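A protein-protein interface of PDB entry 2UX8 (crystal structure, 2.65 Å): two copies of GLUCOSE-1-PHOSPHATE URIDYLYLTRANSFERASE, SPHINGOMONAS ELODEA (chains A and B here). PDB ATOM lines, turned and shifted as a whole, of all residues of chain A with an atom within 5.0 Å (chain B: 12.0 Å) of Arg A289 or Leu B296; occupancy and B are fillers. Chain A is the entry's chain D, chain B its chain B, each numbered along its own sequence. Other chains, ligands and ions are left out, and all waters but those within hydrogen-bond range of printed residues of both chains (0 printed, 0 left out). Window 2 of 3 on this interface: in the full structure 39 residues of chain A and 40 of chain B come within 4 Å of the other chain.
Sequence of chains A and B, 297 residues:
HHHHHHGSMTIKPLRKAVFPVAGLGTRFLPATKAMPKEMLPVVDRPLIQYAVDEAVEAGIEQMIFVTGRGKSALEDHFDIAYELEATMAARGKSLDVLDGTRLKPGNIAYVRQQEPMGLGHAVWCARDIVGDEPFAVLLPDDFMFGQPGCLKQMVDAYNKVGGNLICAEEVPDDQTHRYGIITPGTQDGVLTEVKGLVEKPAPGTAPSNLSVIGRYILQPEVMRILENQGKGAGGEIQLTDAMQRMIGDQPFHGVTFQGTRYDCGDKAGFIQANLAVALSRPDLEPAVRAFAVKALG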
ATOM      1  N   LEU A 279      22.265   4.753  24.312  1.00  0.00           N
ATOM      2  CA  LEU A 279      23.515   5.510  24.343  1.00  0.00           C
ATOM      3  C   LEU A 279      23.340   6.921  24.879  1.00  0.00           C
ATOM      4  O   LEU A 279      24.309   7.568  25.261  1.00  0.00           O
ATOM      5  CB  LEU A 279      24.158   5.567  22.955  1.00  0.00           C
ATOM      6  CG  LEU A 279      24.674   4.226  22.421  1.00  0.00           C
ATOM      7  CD1 LEU A 279      25.051   4.387  20.961  1.00  0.00           C
ATOM      8  CD2 LEU A 279      25.859   3.728  23.251  1.00  0.00           C
ATOM      9  N   LEU A 284      23.187   3.742  31.188  1.00  0.00           N
ATOM     10  CA  LEU A 284      23.301   2.602  30.294  1.00  0.00           C
ATOM     11  C   LEU A 284      24.426   2.715  29.287  1.00  0.00           C
ATOM     12  O   LEU A 284      25.030   1.713  28.916  1.00  0.00           O
ATOM     13  CB  LEU A 284      21.988   2.407  29.534  1.00  0.00           C
ATOM     14  CG  LEU A 284      20.725   2.451  30.383  1.00  0.00           C
ATOM     15  CD1 LEU A 284      19.503   2.330  29.489  1.00  0.00           C
ATOM     16  CD2 LEU A 284      20.778   1.338  31.397  1.00  0.00           C
ATOM     17  N   GLU A 285      24.711   3.934  28.845  1.00  0.00           N
ATOM     18  CA  GLU A 285      25.744   4.154  27.839  1.00  0.00           C
ATOM     19  C   GLU A 285      27.094   3.450  28.056  1.00  0.00           C
ATOM     20  O   GLU A 285      27.605   2.785  27.151  1.00  0.00           O
ATOM     21  CB  GLU A 285      25.967   5.649  27.639  1.00  0.00           C
ATOM     22  CG  GLU A 285      26.816   5.952  26.429  1.00  0.00           C
ATOM     23  CD  GLU A 285      28.194   6.442  26.797  1.00  0.00           C
ATOM     24  OE1 GLU A 285      28.376   7.672  26.888  1.00  0.00           O
ATOM     25  OE2 GLU A 285      29.092   5.603  27.005  1.00  0.00           O
ATOM     26  N   PRO A 286      27.694   3.584  29.249  1.00  0.00           N
ATOM     27  CA  PRO A 286      28.978   2.909  29.448  1.00  0.00           C
ATOM     28  C   PRO A 286      28.925   1.424  29.075  1.00  0.00           C
ATOM     29  O   PRO A 286      29.647   0.978  28.189  1.00  0.00           O
ATOM     30  CB  PRO A 286      29.256   3.126  30.932  1.00  0.00           C
ATOM     31  CG  PRO A 286      28.614   4.443  31.202  1.00  0.00           C
ATOM     32  CD  PRO A 286      27.300   4.327  30.458  1.00  0.00           C
ATOM     33  N   ALA A 287      28.058   0.670  29.745  1.00  0.00           N
ATOM     34  CA  ALA A 287      27.920  -0.764  29.496  1.00  0.00           C
ATOM     35  C   ALA A 287      27.531  -1.093  28.060  1.00  0.00           C
ATOM     36  O   ALA A 287      28.080  -2.017  27.460  1.00  0.00           O
ATOM     37  CB  ALA A 287      26.897  -1.359  30.453  1.00  0.00           C
ATOM     38  N   VAL A 288      26.578  -0.338  27.520  1.00  0.00           N
ATOM     39  CA  VAL A 288      26.097  -0.543  26.159  1.00  0.00           C
ATOM     40  C   VAL A 288      27.180  -0.269  25.125  1.00  0.00           C
ATOM     41  O   VAL A 288      27.410  -1.077  24.227  1.00  0.00           O
ATOM     42  CB  VAL A 288      24.890   0.359  25.871  1.00  0.00           C
ATOM     43  CG1 VAL A 288      24.487   0.251  24.409  1.00  0.00           C
ATOM     44  CG2 VAL A 288      23.735  -0.043  26.770  1.00  0.00           C
ATOM     45  N   ARG A 289      27.842   0.875  25.246  1.00  0.00           N
ATOM     46  CA  ARG A 289      28.910   1.218  24.317  1.00  0.00           C
ATOM     47  C   ARG A 289      30.007   0.159  24.353  1.00  0.00           C
ATOM     48  O   ARG A 289      30.437  -0.344  23.312  1.00  0.00           O
ATOM     49  CB  ARG A 289      29.507   2.574  24.675  1.00  0.00           C
ATOM     50  CG  ARG A 289      30.798   2.890  23.944  1.00  0.00           C
ATOM     51  CD  ARG A 289      31.270   4.269  24.317  1.00  0.00           C
ATOM     52  NE  ARG A 289      30.378   5.292  23.783  1.00  0.00           N
ATOM     53  CZ  ARG A 289      30.374   5.680  22.512  1.00  0.00           C
ATOM     54  NH1 ARG A 289      31.219   5.130  21.651  1.00  0.00           N
ATOM     55  NH2 ARG A 289      29.527   6.616  22.101  1.00  0.00           N
ATOM     56  N   ALA A 290      30.461  -0.170  25.558  1.00  0.00           N
ATOM     57  CA  ALA A 290      31.504  -1.172  25.738  1.00  0.00           C
ATOM     58  C   ALA A 290      31.160  -2.447  24.982  1.00  0.00           C
ATOM     59  O   ALA A 290      32.005  -3.007  24.276  1.00  0.00           O
ATOM     60  CB  ALA A 290      31.684  -1.480  27.216  1.00  0.00           C
ATOM     61  N   PHE A 291      29.919  -2.905  25.138  1.00  0.00           N
ATOM     62  CA  PHE A 291      29.469  -4.120  24.469  1.00  0.00           C
ATOM     63  C   PHE A 291      29.431  -3.920  22.970  1.00  0.00           C
ATOM     64  O   PHE A 291      29.970  -4.716  22.206  1.00  0.00           O
ATOM     65  CB  PHE A 291      28.066  -4.519  24.916  1.00  0.00           C
ATOM     66  CG  PHE A 291      27.524  -5.715  24.180  1.00  0.00           C
ATOM     67  CD1 PHE A 291      27.917  -7.007  24.537  1.00  0.00           C
ATOM     68  CD2 PHE A 291      26.672  -5.549  23.090  1.00  0.00           C
ATOM     69  CE1 PHE A 291      27.474  -8.122  23.813  1.00  0.00           C
ATOM     70  CE2 PHE A 291      26.222  -6.657  22.357  1.00  0.00           C
ATOM     71  CZ  PHE A 291      26.626  -7.947  22.720  1.00  0.00           C
ATOM     72  N   ALA A 292      28.766  -2.851  22.564  1.00  0.00           N
ATOM     73  CA  ALA A 292      28.616  -2.529  21.158  1.00  0.00           C
ATOM     74  C   ALA A 292      29.912  -2.693  20.378  1.00  0.00           C
ATOM     75  O   ALA A 292      29.970  -3.439  19.401  1.00  0.00           O
ATOM     76  CB  ALA A 292      28.099  -1.108  21.015  1.00  0.00           C
ATOM     77  N   VAL A 293      30.965  -2.005  20.804  1.00  0.00           N
ATOM     78  CA  VAL A 293      32.212  -2.116  20.073  1.00  0.00           C
ATOM     79  C   VAL A 293      32.778  -3.528  20.031  1.00  0.00           C
ATOM     80  O   VAL A 293      33.107  -4.020  18.957  1.00  0.00           O
ATOM     81  CB  VAL A 293      33.277  -1.139  20.590  1.00  0.00           C
ATOM     82  CG1 VAL A 293      33.373  -1.188  22.071  1.00  0.00           C
ATOM     83  CG2 VAL A 293      34.597  -1.486  19.997  1.00  0.00           C
ATOM     84  N   LEU A 296      31.179  -5.914  17.733  1.00  0.00           N
ATOM     85  CA  LEU A 296      31.171  -5.420  16.372  1.00  0.00           C
ATOM     86  C   LEU A 296      32.443  -5.690  15.556  1.00  0.00           C
ATOM     87  O   LEU A 296      32.531  -5.307  14.398  1.00  0.00           O
ATOM     88  CB  LEU A 296      30.857  -3.931  16.442  1.00  0.00           C
ATOM     89  CG  LEU A 296      30.220  -3.166  15.286  1.00  0.00           C
ATOM     90  CD1 LEU A 296      29.527  -4.081  14.339  1.00  0.00           C
ATOM     91  CD2 LEU A 296      29.232  -2.184  15.848  1.00  0.00           C
ATOM     92  N   TYR B 262      22.799 -13.307  28.413  1.00  0.00           N
ATOM     93  CA  TYR B 262      22.550 -11.892  28.568  1.00  0.00           C
ATOM     94  C   TYR B 262      21.510 -11.701  29.662  1.00  0.00           C
ATOM     95  O   TYR B 262      20.431 -12.299  29.619  1.00  0.00           O
ATOM     96  CB  TYR B 262      22.065 -11.285  27.253  1.00  0.00           C
ATOM     97  CG  TYR B 262      23.086 -11.349  26.140  1.00  0.00           C
ATOM     98  CD1 TYR B 262      23.081 -12.398  25.221  1.00  0.00           C
ATOM     99  CD2 TYR B 262      24.059 -10.354  25.996  1.00  0.00           C
ATOM    100  CE1 TYR B 262      24.018 -12.451  24.177  1.00  0.00           C
ATOM    101  CE2 TYR B 262      24.999 -10.399  24.958  1.00  0.00           C
ATOM    102  CZ  TYR B 262      24.970 -11.451  24.052  1.00  0.00           C
ATOM    103  OH  TYR B 262      25.879 -11.498  23.018  1.00  0.00           O
ATOM    104  N   ASP B 266      18.355  -6.668  33.526  1.00  0.00           N
ATOM    105  CA  ASP B 266      18.927  -5.334  33.597  1.00  0.00           C
ATOM    106  C   ASP B 266      18.837  -4.642  32.227  1.00  0.00           C
ATOM    107  O   ASP B 266      19.104  -5.253  31.192  1.00  0.00           O
ATOM    108  CB  ASP B 266      20.377  -5.484  34.110  1.00  0.00           C
ATOM    109  CG  ASP B 266      21.409  -4.814  33.223  1.00  0.00           C
ATOM    110  OD1 ASP B 266      21.356  -3.579  33.076  1.00  0.00           O
ATOM    111  OD2 ASP B 266      22.287  -5.522  32.682  1.00  0.00           O
ATOM    112  N   LYS B 267      18.431  -3.378  32.228  1.00  0.00           N
ATOM    113  CA  LYS B 267      18.285  -2.597  31.006  1.00  0.00           C
ATOM    114  C   LYS B 267      19.405  -2.749  29.981  1.00  0.00           C
ATOM    115  O   LYS B 267      19.149  -2.968  28.799  1.00  0.00           O
ATOM    116  CB  LYS B 267      18.128  -1.133  31.381  1.00  0.00           C
ATOM    117  CG  LYS B 267      16.775  -0.611  31.035  1.00  0.00           C
ATOM    118  CD  LYS B 267      16.471   0.677  31.739  1.00  0.00           C
ATOM    119  CE  LYS B 267      15.701   0.425  33.005  1.00  0.00           C
ATOM    120  NZ  LYS B 267      15.129   1.703  33.495  1.00  0.00           N
ATOM    121  N   ALA B 268      20.647  -2.627  30.433  1.00  0.00           N
ATOM    122  CA  ALA B 268      21.786  -2.749  29.536  1.00  0.00           C
ATOM    123  C   ALA B 268      21.843  -4.133  28.885  1.00  0.00           C
ATOM    124  O   ALA B 268      22.124  -4.250  27.691  1.00  0.00           O
ATOM    125  CB  ALA B 268      23.083  -2.462  30.291  1.00  0.00           C
ATOM    126  N   GLY B 269      21.572  -5.173  29.670  1.00  0.00           N
ATOM    127  CA  GLY B 269      21.598  -6.530  29.145  1.00  0.00           C
ATOM    128  C   GLY B 269      20.569  -6.740  28.051  1.00  0.00           C
ATOM    129  O   GLY B 269      20.851  -7.348  27.013  1.00  0.00           O
ATOM    130  N   PHE B 270      19.366  -6.229  28.287  1.00  0.00           N
ATOM    131  CA  PHE B 270      18.270  -6.333  27.329  1.00  0.00           C
ATOM    132  C   PHE B 270      18.672  -5.744  25.978  1.00  0.00           C
ATOM    133  O   PHE B 270      18.420  -6.337  24.931  1.00  0.00           O
ATOM    134  CB  PHE B 270      17.044  -5.593  27.875  1.00  0.00           C
ATOM    135  CG  PHE B 270      15.891  -5.511  26.910  1.00  0.00           C
ATOM    136  CD1 PHE B 270      15.143  -6.644  26.589  1.00  0.00           C
ATOM    137  CD2 PHE B 270      15.543  -4.293  26.334  1.00  0.00           C
ATOM    138  CE1 PHE B 270      14.063  -6.561  25.709  1.00  0.00           C
ATOM    139  CE2 PHE B 270      14.466  -4.202  25.454  1.00  0.00           C
ATOM    140  CZ  PHE B 270      13.724  -5.341  25.142  1.00  0.00           C
ATOM    141  N   ILE B 271      19.302  -4.575  26.010  1.00  0.00           N
ATOM    142  CA  ILE B 271      19.721  -3.910  24.786  1.00  0.00           C
ATOM    143  C   ILE B 271      20.858  -4.664  24.126  1.00  0.00           C
ATOM    144  O   ILE B 271      20.859  -4.861  22.913  1.00  0.00           O
ATOM    145  CB  ILE B 271      20.099  -2.446  25.074  1.00  0.00           C
ATOM    146  CG1 ILE B 271      18.819  -1.662  25.366  1.00  0.00           C
ATOM    147  CG2 ILE B 271      20.810  -1.827  23.884  1.00  0.00           C
ATOM    148  CD1 ILE B 271      19.029  -0.480  26.245  1.00  0.00           C
ATOM    149  N   GLN B 272      21.813  -5.108  24.926  1.00  0.00           N
ATOM    150  CA  GLN B 272      22.927  -5.875  24.395  1.00  0.00           C
ATOM    151  C   GLN B 272      22.402  -7.124  23.694  1.00  0.00           C
ATOM    152  O   GLN B 272      22.867  -7.478  22.614  1.00  0.00           O
ATOM    153  CB  GLN B 272      23.870  -6.282  25.524  1.00  0.00           C
ATOM    154  CG  GLN B 272      24.626  -5.119  26.124  1.00  0.00           C
ATOM    155  CD  GLN B 272      25.411  -5.502  27.360  1.00  0.00           C
ATOM    156  OE1 GLN B 272      25.683  -6.679  27.603  1.00  0.00           O
ATOM    157  NE2 GLN B 272      25.794  -4.502  28.145  1.00  0.00           N
ATOM    158  N   ALA B 273      21.432  -7.791  24.313  1.00  0.00           N
ATOM    159  CA  ALA B 273      20.866  -9.003  23.745  1.00  0.00           C
ATOM    160  C   ALA B 273      20.230  -8.737  22.384  1.00  0.00           C
ATOM    161  O   ALA B 273      20.413  -9.499  21.433  1.00  0.00           O
ATOM    162  CB  ALA B 273      19.836  -9.589  24.702  1.00  0.00           C
ATOM    163  N   LEU B 275      20.911  -6.421  20.332  1.00  0.00           N
ATOM    164  CA  LEU B 275      21.939  -6.101  19.361  1.00  0.00           C
ATOM    165  C   LEU B 275      22.606  -7.376  18.838  1.00  0.00           C
ATOM    166  O   LEU B 275      22.774  -7.552  17.631  1.00  0.00           O
ATOM    167  CB  LEU B 275      22.974  -5.180  20.008  1.00  0.00           C
ATOM    168  CG  LEU B 275      24.045  -4.600  19.088  1.00  0.00           C
ATOM    169  CD1 LEU B 275      23.398  -3.871  17.930  1.00  0.00           C
ATOM    170  CD2 LEU B 275      24.923  -3.661  19.885  1.00  0.00           C
ATOM    171  N   ALA B 276      22.974  -8.264  19.756  1.00  0.00           N
ATOM    172  CA  ALA B 276      23.627  -9.518  19.412  1.00  0.00           C
ATOM    173  C   ALA B 276      22.792 -10.357  18.459  1.00  0.00           C
ATOM    174  O   ALA B 276      23.277 -10.831  17.432  1.00  0.00           O
ATOM    175  CB  ALA B 276      23.914 -10.310  20.671  1.00  0.00           C
ATOM    176  N   LEU B 279      22.552  -8.810  15.013  1.00  0.00           N
ATOM    177  CA  LEU B 279      23.739  -8.994  14.192  1.00  0.00           C
ATOM    178  C   LEU B 279      23.875 -10.412  13.670  1.00  0.00           C
ATOM    179  O   LEU B 279      24.652 -10.664  12.753  1.00  0.00           O
ATOM    180  CB  LEU B 279      25.002  -8.606  14.968  1.00  0.00           C
ATOM    181  CG  LEU B 279      25.159  -7.133  15.374  1.00  0.00           C
ATOM    182  CD1 LEU B 279      26.444  -6.983  16.159  1.00  0.00           C
ATOM    183  CD2 LEU B 279      25.162  -6.216  14.157  1.00  0.00           C
ATOM    184  N   ALA B 287      22.071  -3.504   7.810  1.00  0.00           N
ATOM    185  CA  ALA B 287      21.563  -2.219   8.291  1.00  0.00           C
ATOM    186  C   ALA B 287      21.945  -1.905   9.731  1.00  0.00           C
ATOM    187  O   ALA B 287      22.313  -0.771  10.044  1.00  0.00           O
ATOM    188  CB  ALA B 287      20.044  -2.163   8.146  1.00  0.00           C
ATOM    189  N   VAL B 288      21.848  -2.901  10.607  1.00  0.00           N
ATOM    190  CA  VAL B 288      22.181  -2.700  12.016  1.00  0.00           C
ATOM    191  C   VAL B 288      23.656  -2.383  12.224  1.00  0.00           C
ATOM    192  O   VAL B 288      23.993  -1.420  12.910  1.00  0.00           O
ATOM    193  CB  VAL B 288      21.797  -3.933  12.870  1.00  0.00           C
ATOM    194  CG1 VAL B 288      22.360  -3.787  14.277  1.00  0.00           C
ATOM    195  CG2 VAL B 288      20.284  -4.063  12.932  1.00  0.00           C
ATOM    196  N   ARG B 289      24.531  -3.195  11.637  1.00  0.00           N
ATOM    197  CA  ARG B 289      25.965  -2.962  11.759  1.00  0.00           C
ATOM    198  C   ARG B 289      26.301  -1.556  11.246  1.00  0.00           C
ATOM    199  O   ARG B 289      27.006  -0.796  11.911  1.00  0.00           O
ATOM    200  CB  ARG B 289      26.754  -4.006  10.959  1.00  0.00           C
ATOM    201  CG  ARG B 289      28.263  -3.730  10.899  1.00  0.00           C
ATOM    202  CD  ARG B 289      29.001  -4.799  10.120  1.00  0.00           C
ATOM    203  NE  ARG B 289      28.941  -6.090  10.794  1.00  0.00           N
ATOM    204  CZ  ARG B 289      29.773  -6.476  11.758  1.00  0.00           C
ATOM    205  NH1 ARG B 289      30.745  -5.670  12.166  1.00  0.00           N
ATOM    206  NH2 ARG B 289      29.629  -7.669  12.320  1.00  0.00           N
ATOM    207  N   ALA B 290      25.784  -1.223  10.065  1.00  0.00           N
ATOM    208  CA  ALA B 290      26.008   0.083   9.448  1.00  0.00           C
ATOM    209  C   ALA B 290      25.693   1.218  10.413  1.00  0.00           C
ATOM    210  O   ALA B 290      26.480   2.150  10.573  1.00  0.00           O
ATOM    211  CB  ALA B 290      25.143   0.220   8.200  1.00  0.00           C
ATOM    212  N   PHE B 291      24.531   1.139  11.052  1.00  0.00           N
ATOM    213  CA  PHE B 291      24.113   2.165  11.997  1.00  0.00           C
ATOM    214  C   PHE B 291      24.960   2.150  13.246  1.00  0.00           C
ATOM    215  O   PHE B 291      25.410   3.193  13.706  1.00  0.00           O
ATOM    216  CB  PHE B 291      22.662   1.974  12.420  1.00  0.00           C
ATOM    217  CG  PHE B 291      22.212   2.950  13.477  1.00  0.00           C
ATOM    218  CD1 PHE B 291      21.780   4.228  13.128  1.00  0.00           C
ATOM    219  CD2 PHE B 291      22.247   2.597  14.825  1.00  0.00           C
ATOM    220  CE1 PHE B 291      21.384   5.144  14.107  1.00  0.00           C
ATOM    221  CE2 PHE B 291      21.855   3.505  15.812  1.00  0.00           C
ATOM    222  CZ  PHE B 291      21.421   4.782  15.452  1.00  0.00           C
ATOM    223  N   ALA B 292      25.147   0.964  13.810  1.00  0.00           N
ATOM    224  CA  ALA B 292      25.938   0.814  15.025  1.00  0.00           C
ATOM    225  C   ALA B 292      27.258   1.562  14.904  1.00  0.00           C
ATOM    226  O   ALA B 292      27.607   2.365  15.768  1.00  0.00           O
ATOM    227  CB  ALA B 292      26.197  -0.662  15.296  1.00  0.00           C
ATOM    228  N   VAL B 293      27.981   1.298  13.820  1.00  0.00           N
ATOM    229  CA  VAL B 293      29.271   1.936  13.566  1.00  0.00           C
ATOM    230  C   VAL B 293      29.170   3.463  13.609  1.00  0.00           C
ATOM    231  O   VAL B 293      29.862   4.116  14.393  1.00  0.00           O
ATOM    232  CB  VAL B 293      29.837   1.493  12.197  1.00  0.00           C
ATOM    233  CG1 VAL B 293      31.136   2.214  11.903  1.00  0.00           C
ATOM    234  CG2 VAL B 293      30.068  -0.004  12.199  1.00  0.00           C
ATOM    235  N   LYS B 294      28.307   4.023  12.765  1.00  0.00           N
ATOM    236  CA  LYS B 294      28.104   5.469  12.713  1.00  0.00           C
ATOM    237  C   LYS B 294      27.842   6.038  14.096  1.00  0.00           C
ATOM    238  O   LYS B 294      28.568   6.902  14.592  1.00  0.00           O
ATOM    239  CB  LYS B 294      26.882   5.816  11.873  1.00  0.00           C
ATOM    240  CG  LYS B 294      27.021   5.683  10.393  1.00  0.00           C
ATOM    241  CD  LYS B 294      25.861   6.420   9.750  1.00  0.00           C
ATOM    242  CE  LYS B 294      25.924   6.397   8.242  1.00  0.00           C
ATOM    243  NZ  LYS B 294      25.603   5.057   7.695  1.00  0.00           N
ATOM    244  N   ALA B 295      26.763   5.546  14.693  1.00  0.00           N
ATOM    245  CA  ALA B 295      26.307   5.974  16.005  1.00  0.00           C
ATOM    246  C   ALA B 295      27.347   5.910  17.124  1.00  0.00           C
ATOM    247  O   ALA B 295      27.199   6.574  18.144  1.00  0.00           O
ATOM    248  CB  ALA B 295      25.079   5.166  16.393  1.00  0.00           C
ATOM    249  N   LEU B 296      28.401   5.125  16.938  1.00  0.00           N
ATOM    250  CA  LEU B 296      29.425   4.993  17.965  1.00  0.00           C
ATOM    251  C   LEU B 296      30.582   5.985  17.909  1.00  0.00           C
ATOM    252  O   LEU B 296      31.366   6.056  18.845  1.00  0.00           O
ATOM    253  CB  LEU B 296      30.015   3.587  17.942  1.00  0.00           C
ATOM    254  CG  LEU B 296      29.226   2.435  18.550  1.00  0.00           C
ATOM    255  CD1 LEU B 296      29.959   1.144  18.275  1.00  0.00           C
ATOM    256  CD2 LEU B 296      29.068   2.639  20.039  1.00  0.00           C
ATOM    257  N   GLY B 297      30.709   6.742  16.827  1.00  0.00           N
ATOM    258  CA  GLY B 297      31.815   7.679  16.733  1.00  0.00           C
ATOM    259  C   GLY B 297      33.009   6.995  16.100  1.00  0.00           C
ATOM    260  O   GLY B 297      32.943   5.807  15.776  1.00  0.00           O
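The backbone NH (N) of Ala B268 sits at hydrogen-bond distance from the side-chain carboxylate (OD1) of Asp B266 (2.9 Å). NE of Arg A289 lies within salt-bridge range of OE2 of Glu A285 (3.5 Å).
Of the 12 printed residues of chain A, 6 touch a printed residue of chain B. Among the printed residues, no Asp or Glu carboxylate lies within 4 Å of a Lys or Arg side-chain nitrogen of the other chain.
Lys B267 touches Leu A284. Ala B268 touches Ala A287 (CB to CB, 3.97 Å). Phe A291 touches Tyr B262 (CE1 to CE2, 3.6 Å). Phe A291 touches Gln B272. CD2 of Leu B296 touches CB of Ala A292, 3.99 Å away. CB of Ala B292 touches CD2 of Leu A296, at 3.4 Å.
The backbone carbonyl oxygen of Ala A287 sits at hydrogen-bond distance from the side-chain amide nitrogen of Gln B272, 3.4 Å away. NH1 of Arg B289 lies within hydrogen-bond range of O of Leu A296 (2.9 Å). O of Leu B296 sits at hydrogen-bond distance from NH1 of Arg A289 (3.0 Å).
Of chain B, only Leu B296 (3.0 Å) comes within 4 Å of Arg A289. Printed residues of chain A within 4 Å of Leu B296: Arg A289 and Ala A292. Leu A279 touches none of the printed residues of chain B. No residue of chain B comes within 4 Å of Glu A285. Of chain B, only Ala B268 and Gln B272 come within 4 Å of Ala A287. No residue of chain B comes within 4 Å of Val A288. No residue of chain B comes within 4 Å of Ala A290. No residue of chain B comes within 4 Å of Val A293. Of the printed residues of chain A, Lys B267 touches Leu A284 (3.6 Å). Of the printed residues of chain A, Ala B292 touches Leu A296 (3.4 Å). Of the printed residues of chain B, Ala A292 touches Leu B296. Of the printed residues of chain A, Tyr B262 touches Phe A291 (3.6 Å). Printed residues of chain A within 4 Å of Arg B289: Leu A296. Ala B276 touches none of the printed residues of chain A. The nearest residue of chain B that does not touch Arg A289 is Ala B295 (4.6 Å). The nearest printed residue of chain A that does not touch Leu B296 is Val A293 (4.2 Å).
Arg A289 touches Leu B296, and with the chains exchanged Leu A296 touches Arg B289. Ala A292 touches Leu B296, and with the chains exchanged Leu A296 touches Ala B292.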
